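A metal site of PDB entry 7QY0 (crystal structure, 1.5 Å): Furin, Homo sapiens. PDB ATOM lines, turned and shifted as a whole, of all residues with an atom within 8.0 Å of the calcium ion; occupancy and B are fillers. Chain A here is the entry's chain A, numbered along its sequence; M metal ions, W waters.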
ATOM      1  N   GLY A 148      18.481 -10.975 -30.647  1.00  0.00           N
ATOM      2  CA  GLY A 148      18.262 -11.968 -29.622  1.00  0.00           C
ATOM      3  C   GLY A 148      17.352 -13.072 -30.131  1.00  0.00           C
ATOM      4  O   GLY A 148      17.366 -13.412 -31.322  1.00  0.00           O
ATOM      5  N   PRO A 149      16.532 -13.629 -29.240  1.00  0.00           N
ATOM      6  CA  PRO A 149      15.536 -14.618 -29.669  1.00  0.00           C
ATOM      7  C   PRO A 149      14.564 -14.004 -30.667  1.00  0.00           C
ATOM      8  O   PRO A 149      14.423 -12.795 -30.778  1.00  0.00           O
ATOM      9  CB  PRO A 149      14.810 -15.011 -28.381  1.00  0.00           C
ATOM     10  CG  PRO A 149      15.496 -14.329 -27.296  1.00  0.00           C
ATOM     11  CD  PRO A 149      16.375 -13.266 -27.824  1.00  0.00           C
ATOM     12  N   GLU A 150      13.880 -14.885 -31.398  1.00  0.00           N
ATOM     13  CA  GLU A 150      13.005 -14.441 -32.488  1.00  0.00           C
ATOM     14  C   GLU A 150      12.006 -13.410 -31.997  1.00  0.00           C
ATOM     15  O   GLU A 150      11.372 -13.573 -30.951  1.00  0.00           O
ATOM     16  CB  GLU A 150      12.258 -15.630 -33.084  1.00  0.00           C
ATOM     17  CG  GLU A 150      13.124 -16.499 -33.947  1.00  0.00           C
ATOM     18  CD  GLU A 150      13.108 -16.102 -35.416  1.00  0.00           C
ATOM     19  OE1 GLU A 150      13.273 -17.005 -36.239  1.00  0.00           O
ATOM     20  OE2 GLU A 150      12.940 -14.904 -35.746  1.00  0.00           O
ATOM     21  N   ASP A 151      11.847 -12.358 -32.790  1.00  0.00           N
ATOM     22  CA  ASP A 151      10.901 -11.274 -32.528  1.00  0.00           C
ATOM     23  C   ASP A 151       9.536 -11.588 -33.159  1.00  0.00           C
ATOM     24  O   ASP A 151       8.940 -10.764 -33.864  1.00  0.00           O
ATOM     25  CB  ASP A 151      11.478  -9.956 -33.046  1.00  0.00           C
ATOM     26  CG  ASP A 151      12.568  -9.382 -32.134  1.00  0.00           C
ATOM     27  OD1 ASP A 151      12.606  -9.736 -30.934  1.00  0.00           O
ATOM     28  OD2 ASP A 151      13.358  -8.533 -32.618  1.00  0.00           O
ATOM     29  N   ASP A 152       9.051 -12.803 -32.932  1.00  0.00           N
ATOM     30  CA  ASP A 152       7.779 -13.226 -33.525  1.00  0.00           C
ATOM     31  C   ASP A 152       6.590 -12.977 -32.617  1.00  0.00           C
ATOM     32  O   ASP A 152       5.449 -13.248 -33.029  1.00  0.00           O
ATOM     33  CB  ASP A 152       7.817 -14.722 -33.936  1.00  0.00           C
ATOM     34  CG  ASP A 152       8.179 -15.655 -32.794  1.00  0.00           C
ATOM     35  OD1 ASP A 152       8.275 -15.211 -31.638  1.00  0.00           O
ATOM     36  OD2 ASP A 152       8.375 -16.868 -33.082  1.00  0.00           O
ATOM     37  N   GLY A 153       6.803 -12.441 -31.423  1.00  0.00           N
ATOM     38  CA  GLY A 153       5.703 -12.186 -30.525  1.00  0.00           C
ATOM     39  C   GLY A 153       5.148 -13.424 -29.866  1.00  0.00           C
ATOM     40  O   GLY A 153       4.072 -13.351 -29.257  1.00  0.00           O
ATOM     41  N   LYS A 154       5.836 -14.556 -29.969  1.00  0.00           N
ATOM     42  CA  LYS A 154       5.401 -15.755 -29.284  1.00  0.00           C
ATOM     43  C   LYS A 154       6.524 -16.507 -28.577  1.00  0.00           C
ATOM     44  O   LYS A 154       6.270 -17.553 -27.983  1.00  0.00           O
ATOM     45  CB  LYS A 154       4.686 -16.694 -30.257  1.00  0.00           C
ATOM     46  CG  LYS A 154       5.407 -17.006 -31.540  1.00  0.00           C
ATOM     47  CD  LYS A 154       4.464 -17.785 -32.455  1.00  0.00           C
ATOM     48  CE  LYS A 154       5.121 -18.108 -33.777  1.00  0.00           C
ATOM     49  N   THR A 155       7.743 -15.996 -28.597  1.00  0.00           N
ATOM     50  CA  THR A 155       8.892 -16.667 -28.001  1.00  0.00           C
ATOM     51  C   THR A 155       9.168 -16.092 -26.615  1.00  0.00           C
ATOM     52  O   THR A 155       9.110 -14.865 -26.418  1.00  0.00           O
ATOM     53  CB  THR A 155      10.105 -16.502 -28.923  1.00  0.00           C
ATOM     54  OG1 THR A 155       9.807 -17.092 -30.202  1.00  0.00           O
ATOM     55  CG2 THR A 155      11.355 -17.174 -28.368  1.00  0.00           C
ATOM     56  N   ALA A 185      19.899  -4.024 -28.014  1.00  0.00           N
ATOM     57  CA  ALA A 185      18.690  -3.520 -28.642  1.00  0.00           C
ATOM     58  C   ALA A 185      17.482  -4.237 -28.046  1.00  0.00           C
ATOM     59  O   ALA A 185      17.481  -5.463 -27.898  1.00  0.00           O
ATOM     60  CB  ALA A 185      18.749  -3.753 -30.155  1.00  0.00           C
ATOM     61  N   SER A 186      16.433  -3.478 -27.724  1.00  0.00           N
ATOM     62  CA  SER A 186      15.287  -4.094 -27.060  1.00  0.00           C
ATOM     63  C   SER A 186      14.384  -4.889 -28.000  1.00  0.00           C
ATOM     64  O   SER A 186      13.496  -5.603 -27.519  1.00  0.00           O
ATOM     65  CB  SER A 186      14.463  -3.029 -26.341  1.00  0.00           C
ATOM     66  OG  SER A 186      13.937  -2.105 -27.270  1.00  0.00           O
ATOM     67  N   GLY A 187      14.567  -4.786 -29.313  1.00  0.00           N
ATOM     68  CA  GLY A 187      13.844  -5.665 -30.220  1.00  0.00           C
ATOM     69  C   GLY A 187      13.169  -4.990 -31.389  1.00  0.00           C
ATOM     70  O   GLY A 187      12.924  -3.777 -31.365  1.00  0.00           O
ATOM     71  N   ASN A 188      12.860  -5.772 -32.431  1.00  0.00           N
ATOM     72  CA  ASN A 188      12.178  -5.262 -33.629  1.00  0.00           C
ATOM     73  C   ASN A 188      10.771  -5.855 -33.808  1.00  0.00           C
ATOM     74  O   ASN A 188      10.218  -5.785 -34.909  1.00  0.00           O
ATOM     75  CB  ASN A 188      12.991  -5.556 -34.897  1.00  0.00           C
ATOM     76  CG  ASN A 188      14.301  -4.800 -34.955  1.00  0.00           C
ATOM     77  OD1 ASN A 188      14.376  -3.608 -34.651  1.00  0.00           O
ATOM     78  ND2 ASN A 188      15.351  -5.501 -35.357  1.00  0.00           N
ATOM     79  N   GLY A 189      10.194  -6.425 -32.758  1.00  0.00           N
ATOM     80  CA  GLY A 189       8.941  -7.155 -32.881  1.00  0.00           C
ATOM     81  C   GLY A 189       7.643  -6.383 -32.751  1.00  0.00           C
ATOM     82  O   GLY A 189       6.585  -6.984 -32.515  1.00  0.00           O
ATOM     83  N   GLY A 190       7.678  -5.063 -32.954  1.00  0.00           N
ATOM     84  CA  GLY A 190       6.482  -4.257 -32.761  1.00  0.00           C
ATOM     85  C   GLY A 190       5.272  -4.705 -33.555  1.00  0.00           C
ATOM     86  O   GLY A 190       4.148  -4.714 -33.060  1.00  0.00           O
ATOM     87  N   HIS A 193       3.362  -7.396 -32.075  1.00  0.00           N
ATOM     88  CA  HIS A 193       2.925  -7.101 -30.697  1.00  0.00           C
ATOM     89  C   HIS A 193       3.807  -7.801 -29.676  1.00  0.00           C
ATOM     90  O   HIS A 193       3.349  -8.264 -28.638  1.00  0.00           O
ATOM     91  CB  HIS A 193       1.444  -7.448 -30.522  1.00  0.00           C
ATOM     92  CG  HIS A 193       0.577  -6.833 -31.570  1.00  0.00           C
ATOM     93  ND1 HIS A 193       0.372  -5.476 -31.661  1.00  0.00           N
ATOM     94  CD2 HIS A 193      -0.076  -7.391 -32.629  1.00  0.00           C
ATOM     95  CE1 HIS A 193      -0.394  -5.214 -32.715  1.00  0.00           C
ATOM     96  NE2 HIS A 193      -0.682  -6.362 -33.310  1.00  0.00           N
ATOM     97  N   ASP A 194       5.104  -7.889 -29.985  1.00  0.00           N
ATOM     98  CA  ASP A 194       6.050  -8.485 -29.051  1.00  0.00           C
ATOM     99  C   ASP A 194       6.222  -7.552 -27.848  1.00  0.00           C
ATOM    100  O   ASP A 194       6.010  -6.348 -27.934  1.00  0.00           O
ATOM    101  CB  ASP A 194       7.378  -8.748 -29.751  1.00  0.00           C
ATOM    102  CG  ASP A 194       8.207  -9.814 -29.058  1.00  0.00           C
ATOM    103  OD1 ASP A 194       7.784 -10.348 -28.006  1.00  0.00           O
ATOM    104  OD2 ASP A 194       9.320 -10.122 -29.587  1.00  0.00           O
ATOM    105  N   SER A 195       6.584  -8.152 -26.714  1.00  0.00           N
ATOM    106  CA  SER A 195       6.680  -7.488 -25.412  1.00  0.00           C
ATOM    107  C   SER A 195       8.042  -7.877 -24.860  1.00  0.00           C
ATOM    108  O   SER A 195       8.278  -9.060 -24.584  1.00  0.00           O
ATOM    109  CB  SER A 195       5.515  -7.959 -24.518  1.00  0.00           C
ATOM    110  OG  SER A 195       5.399  -7.254 -23.287  1.00  0.00           O
ATOM    111  N   CYS A 196       8.970  -6.930 -24.751  1.00  0.00           N
ATOM    112  CA  CYS A 196      10.372  -7.342 -24.774  1.00  0.00           C
ATOM    113  C   CYS A 196      10.937  -7.883 -23.453  1.00  0.00           C
ATOM    114  O   CYS A 196      12.090  -8.308 -23.441  1.00  0.00           O
ATOM    115  CB  CYS A 196      11.278  -6.204 -25.289  1.00  0.00           C
ATOM    116  SG  CYS A 196      10.901  -4.470 -24.807  1.00  0.00           S
ATOM    117  N   ASN A 197      10.186  -7.904 -22.338  1.00  0.00           N
ATOM    118  CA  ASN A 197      10.727  -8.657 -21.197  1.00  0.00           C
ATOM    119  C   ASN A 197      10.741 -10.158 -21.457  1.00  0.00           C
ATOM    120  O   ASN A 197      11.323 -10.928 -20.658  1.00  0.00           O
ATOM    121  CB  ASN A 197       9.925  -8.384 -19.910  1.00  0.00           C
ATOM    122  CG  ASN A 197      10.073  -6.954 -19.387  1.00  0.00           C
ATOM    123  OD1 ASN A 197      10.991  -6.207 -19.758  1.00  0.00           O
ATOM    124  ND2 ASN A 197       9.162  -6.576 -18.490  1.00  0.00           N
ATOM    125  N   CYS A 198      10.106 -10.626 -22.544  1.00  0.00           N
ATOM    126  CA  CYS A 198      10.173 -12.020 -22.956  1.00  0.00           C
ATOM    127  C   CYS A 198      11.474 -12.358 -23.669  1.00  0.00           C
ATOM    128  O   CYS A 198      11.656 -13.509 -24.072  1.00  0.00           O
ATOM    129  CB  CYS A 198       8.994 -12.352 -23.875  1.00  0.00           C
ATOM    130  SG  CYS A 198       7.388 -12.253 -23.046  1.00  0.00           S
ATOM    131  N   ASP A 199      12.356 -11.383 -23.849  1.00  0.00           N
ATOM    132  CA  ASP A 199      13.705 -11.537 -24.392  1.00  0.00           C
ATOM    133  C   ASP A 199      14.670 -11.411 -23.213  1.00  0.00           C
ATOM    134  O   ASP A 199      14.857 -10.319 -22.675  1.00  0.00           O
ATOM    135  CB  ASP A 199      13.905 -10.473 -25.478  1.00  0.00           C
ATOM    136  CG  ASP A 199      15.341 -10.295 -25.946  1.00  0.00           C
ATOM    137  OD1 ASP A 199      16.305 -10.783 -25.309  1.00  0.00           O
ATOM    138  OD2 ASP A 199      15.498  -9.604 -26.991  1.00  0.00           O
ATOM    139  N   GLY A 200      15.252 -12.545 -22.804  1.00  0.00           N
ATOM    140  CA  GLY A 200      16.070 -12.564 -21.598  1.00  0.00           C
ATOM    141  C   GLY A 200      17.386 -11.843 -21.725  1.00  0.00           C
ATOM    142  O   GLY A 200      18.058 -11.610 -20.705  1.00  0.00           O
ATOM    143  N   THR A 202      17.742  -8.635 -23.426  1.00  0.00           N
ATOM    144  CA  THR A 202      17.412  -7.254 -23.099  1.00  0.00           C
ATOM    145  C   THR A 202      16.803  -7.139 -21.698  1.00  0.00           C
ATOM    146  O   THR A 202      17.012  -6.133 -21.017  1.00  0.00           O
ATOM    147  CB  THR A 202      16.504  -6.676 -24.196  1.00  0.00           C
ATOM    148  OG1 THR A 202      16.505  -5.251 -24.098  1.00  0.00           O
ATOM    149  CG2 THR A 202      15.064  -7.210 -24.139  1.00  0.00           C
ATOM    150  N   TYR A 222       8.271  -0.798 -35.407  1.00  0.00           N
ATOM    151  CA  TYR A 222       8.976  -2.007 -34.997  1.00  0.00           C
ATOM    152  C   TYR A 222       9.285  -2.060 -33.506  1.00  0.00           C
ATOM    153  O   TYR A 222       9.771  -3.083 -33.030  1.00  0.00           O
ATOM    154  CB  TYR A 222      10.281  -2.143 -35.799  1.00  0.00           C
ATOM    155  CG  TYR A 222      11.134  -0.897 -35.786  1.00  0.00           C
ATOM    156  CD1 TYR A 222      11.917  -0.597 -34.683  1.00  0.00           C
ATOM    157  CD2 TYR A 222      11.132  -0.012 -36.855  1.00  0.00           C
ATOM    158  CE1 TYR A 222      12.670   0.543 -34.644  1.00  0.00           C
ATOM    159  CE2 TYR A 222      11.897   1.126 -36.825  1.00  0.00           C
ATOM    160  CZ  TYR A 222      12.661   1.408 -35.709  1.00  0.00           C
ATOM    161  OH  TYR A 222      13.417   2.544 -35.628  1.00  0.00           O
ATOM    162  N   GLU A 224       9.287  -2.490 -29.512  1.00  0.00           N
ATOM    163  CA  GLU A 224       8.701  -3.296 -28.435  1.00  0.00           C
ATOM    164  C   GLU A 224       8.739  -2.483 -27.154  1.00  0.00           C
ATOM    165  O   GLU A 224       9.777  -1.915 -26.803  1.00  0.00           O
ATOM    166  CB  GLU A 224       9.468  -4.616 -28.236  1.00  0.00           C
ATOM    167  CG  GLU A 224       9.487  -5.517 -29.471  1.00  0.00           C
ATOM    168  CD  GLU A 224      10.207  -6.838 -29.252  1.00  0.00           C
ATOM    169  OE1 GLU A 224      10.098  -7.440 -28.154  1.00  0.00           O
ATOM    170  OE2 GLU A 224      10.885  -7.305 -30.203  1.00  0.00           O
ATOM    171  N   CYS A 226       8.627  -2.450 -23.068  1.00  0.00           N
ATOM    172  CA  CYS A 226       8.753  -3.274 -21.872  1.00  0.00           C
ATOM    173  C   CYS A 226       9.433  -2.463 -20.769  1.00  0.00           C
ATOM    174  O   CYS A 226      10.063  -1.442 -21.028  1.00  0.00           O
ATOM    175  CB  CYS A 226       9.520  -4.570 -22.141  1.00  0.00           C
ATOM    176  SG  CYS A 226      11.197  -4.394 -22.795  1.00  0.00           S
ATOM    177  N   ARG A 412       0.164 -10.689 -25.676  1.00  0.00           N
ATOM    178  CA  ARG A 412       0.842 -11.042 -26.926  1.00  0.00           C
ATOM    179  C   ARG A 412      -0.098 -11.936 -27.719  1.00  0.00           C
ATOM    180  O   ARG A 412      -0.163 -13.150 -27.468  1.00  0.00           O
ATOM    181  CB  ARG A 412       2.177 -11.736 -26.640  1.00  0.00           C
ATOM    182  CG  ARG A 412       3.233 -10.797 -26.009  1.00  0.00           C
ATOM    183  CD  ARG A 412       4.672 -11.294 -26.296  1.00  0.00           C
ATOM    184  NE  ARG A 412       4.882 -12.675 -25.851  1.00  0.00           N
ATOM    185  CZ  ARG A 412       5.941 -13.399 -26.151  1.00  0.00           C
ATOM    186  NH1 ARG A 412       6.915 -12.902 -26.915  1.00  0.00           N
ATOM    187  NH2 ARG A 412       6.038 -14.654 -25.704  1.00  0.00           N
HETATM  188 CA    CA M   1      11.404  -9.340 -28.922  1.00  0.00          CA
HETATM  189  O   HOH W   1      12.419 -11.593 -28.766  1.00  0.00           O
HETATM  190  O   HOH W   2      13.264  -8.332 -27.815  1.00  0.00           O
HETATM  191  O   HOH W   3      10.531 -10.294 -26.841  1.00  0.00           O
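SG of Cys 226 is disulfide-bonded to SG of Cys 196, 2.0 Å away.
The guanidinium group (NH1) of Arg 412 lies within salt-bridge range of the side-chain carboxylate (OD1) of Asp 194 (2.9 Å).
The backbone NH (N) of Asn 188 lies within hydrogen-bond range of the side-chain carboxylate (OD2) of Asp 151, at 2.8 Å.
The backbone NH (N) of Gly 189 sits close to the side-chain carboxylate (OE2) of Glu 224 (2.8 Å).
The backbone NH (N) of Asp 194 is in hydrogen-bond range of the backbone carbonyl oxygen (O) of Gly 189 (3.1 Å).
N of Asn 188 sits close to OE2 of Glu 224.
Water W2 bridges the side-chain carboxylate (OD2) of Asp 199 (2.7 Å) and the backbone carbonyl oxygen (O) of Ser 186 (2.8 Å).
Water W3 bridges the side-chain carboxylate of Asp 194 (3.0 Å) and the backbone carbonyl oxygen of Ser 195 (3.4 Å).
The side-chain carboxylate (OD2) of Asp 194 is bound to the calcium ion (2.3 Å).
The calcium ion is bound by the side-chain carboxylate (OD1) of Asp 151 (2.4 Å).
The calcium ion is bound by water W2.
The calcium ion is bound by the side-chain carboxylate (OE1) of Glu 224 (2.4 Å).
The calcium ion is bound by water W3 (2.5 Å).
The calcium ion is bound by the side-chain carboxylate (OE2) of Glu 224 (2.5 Å).
Water W1 binds the calcium ion (2.5 Å).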
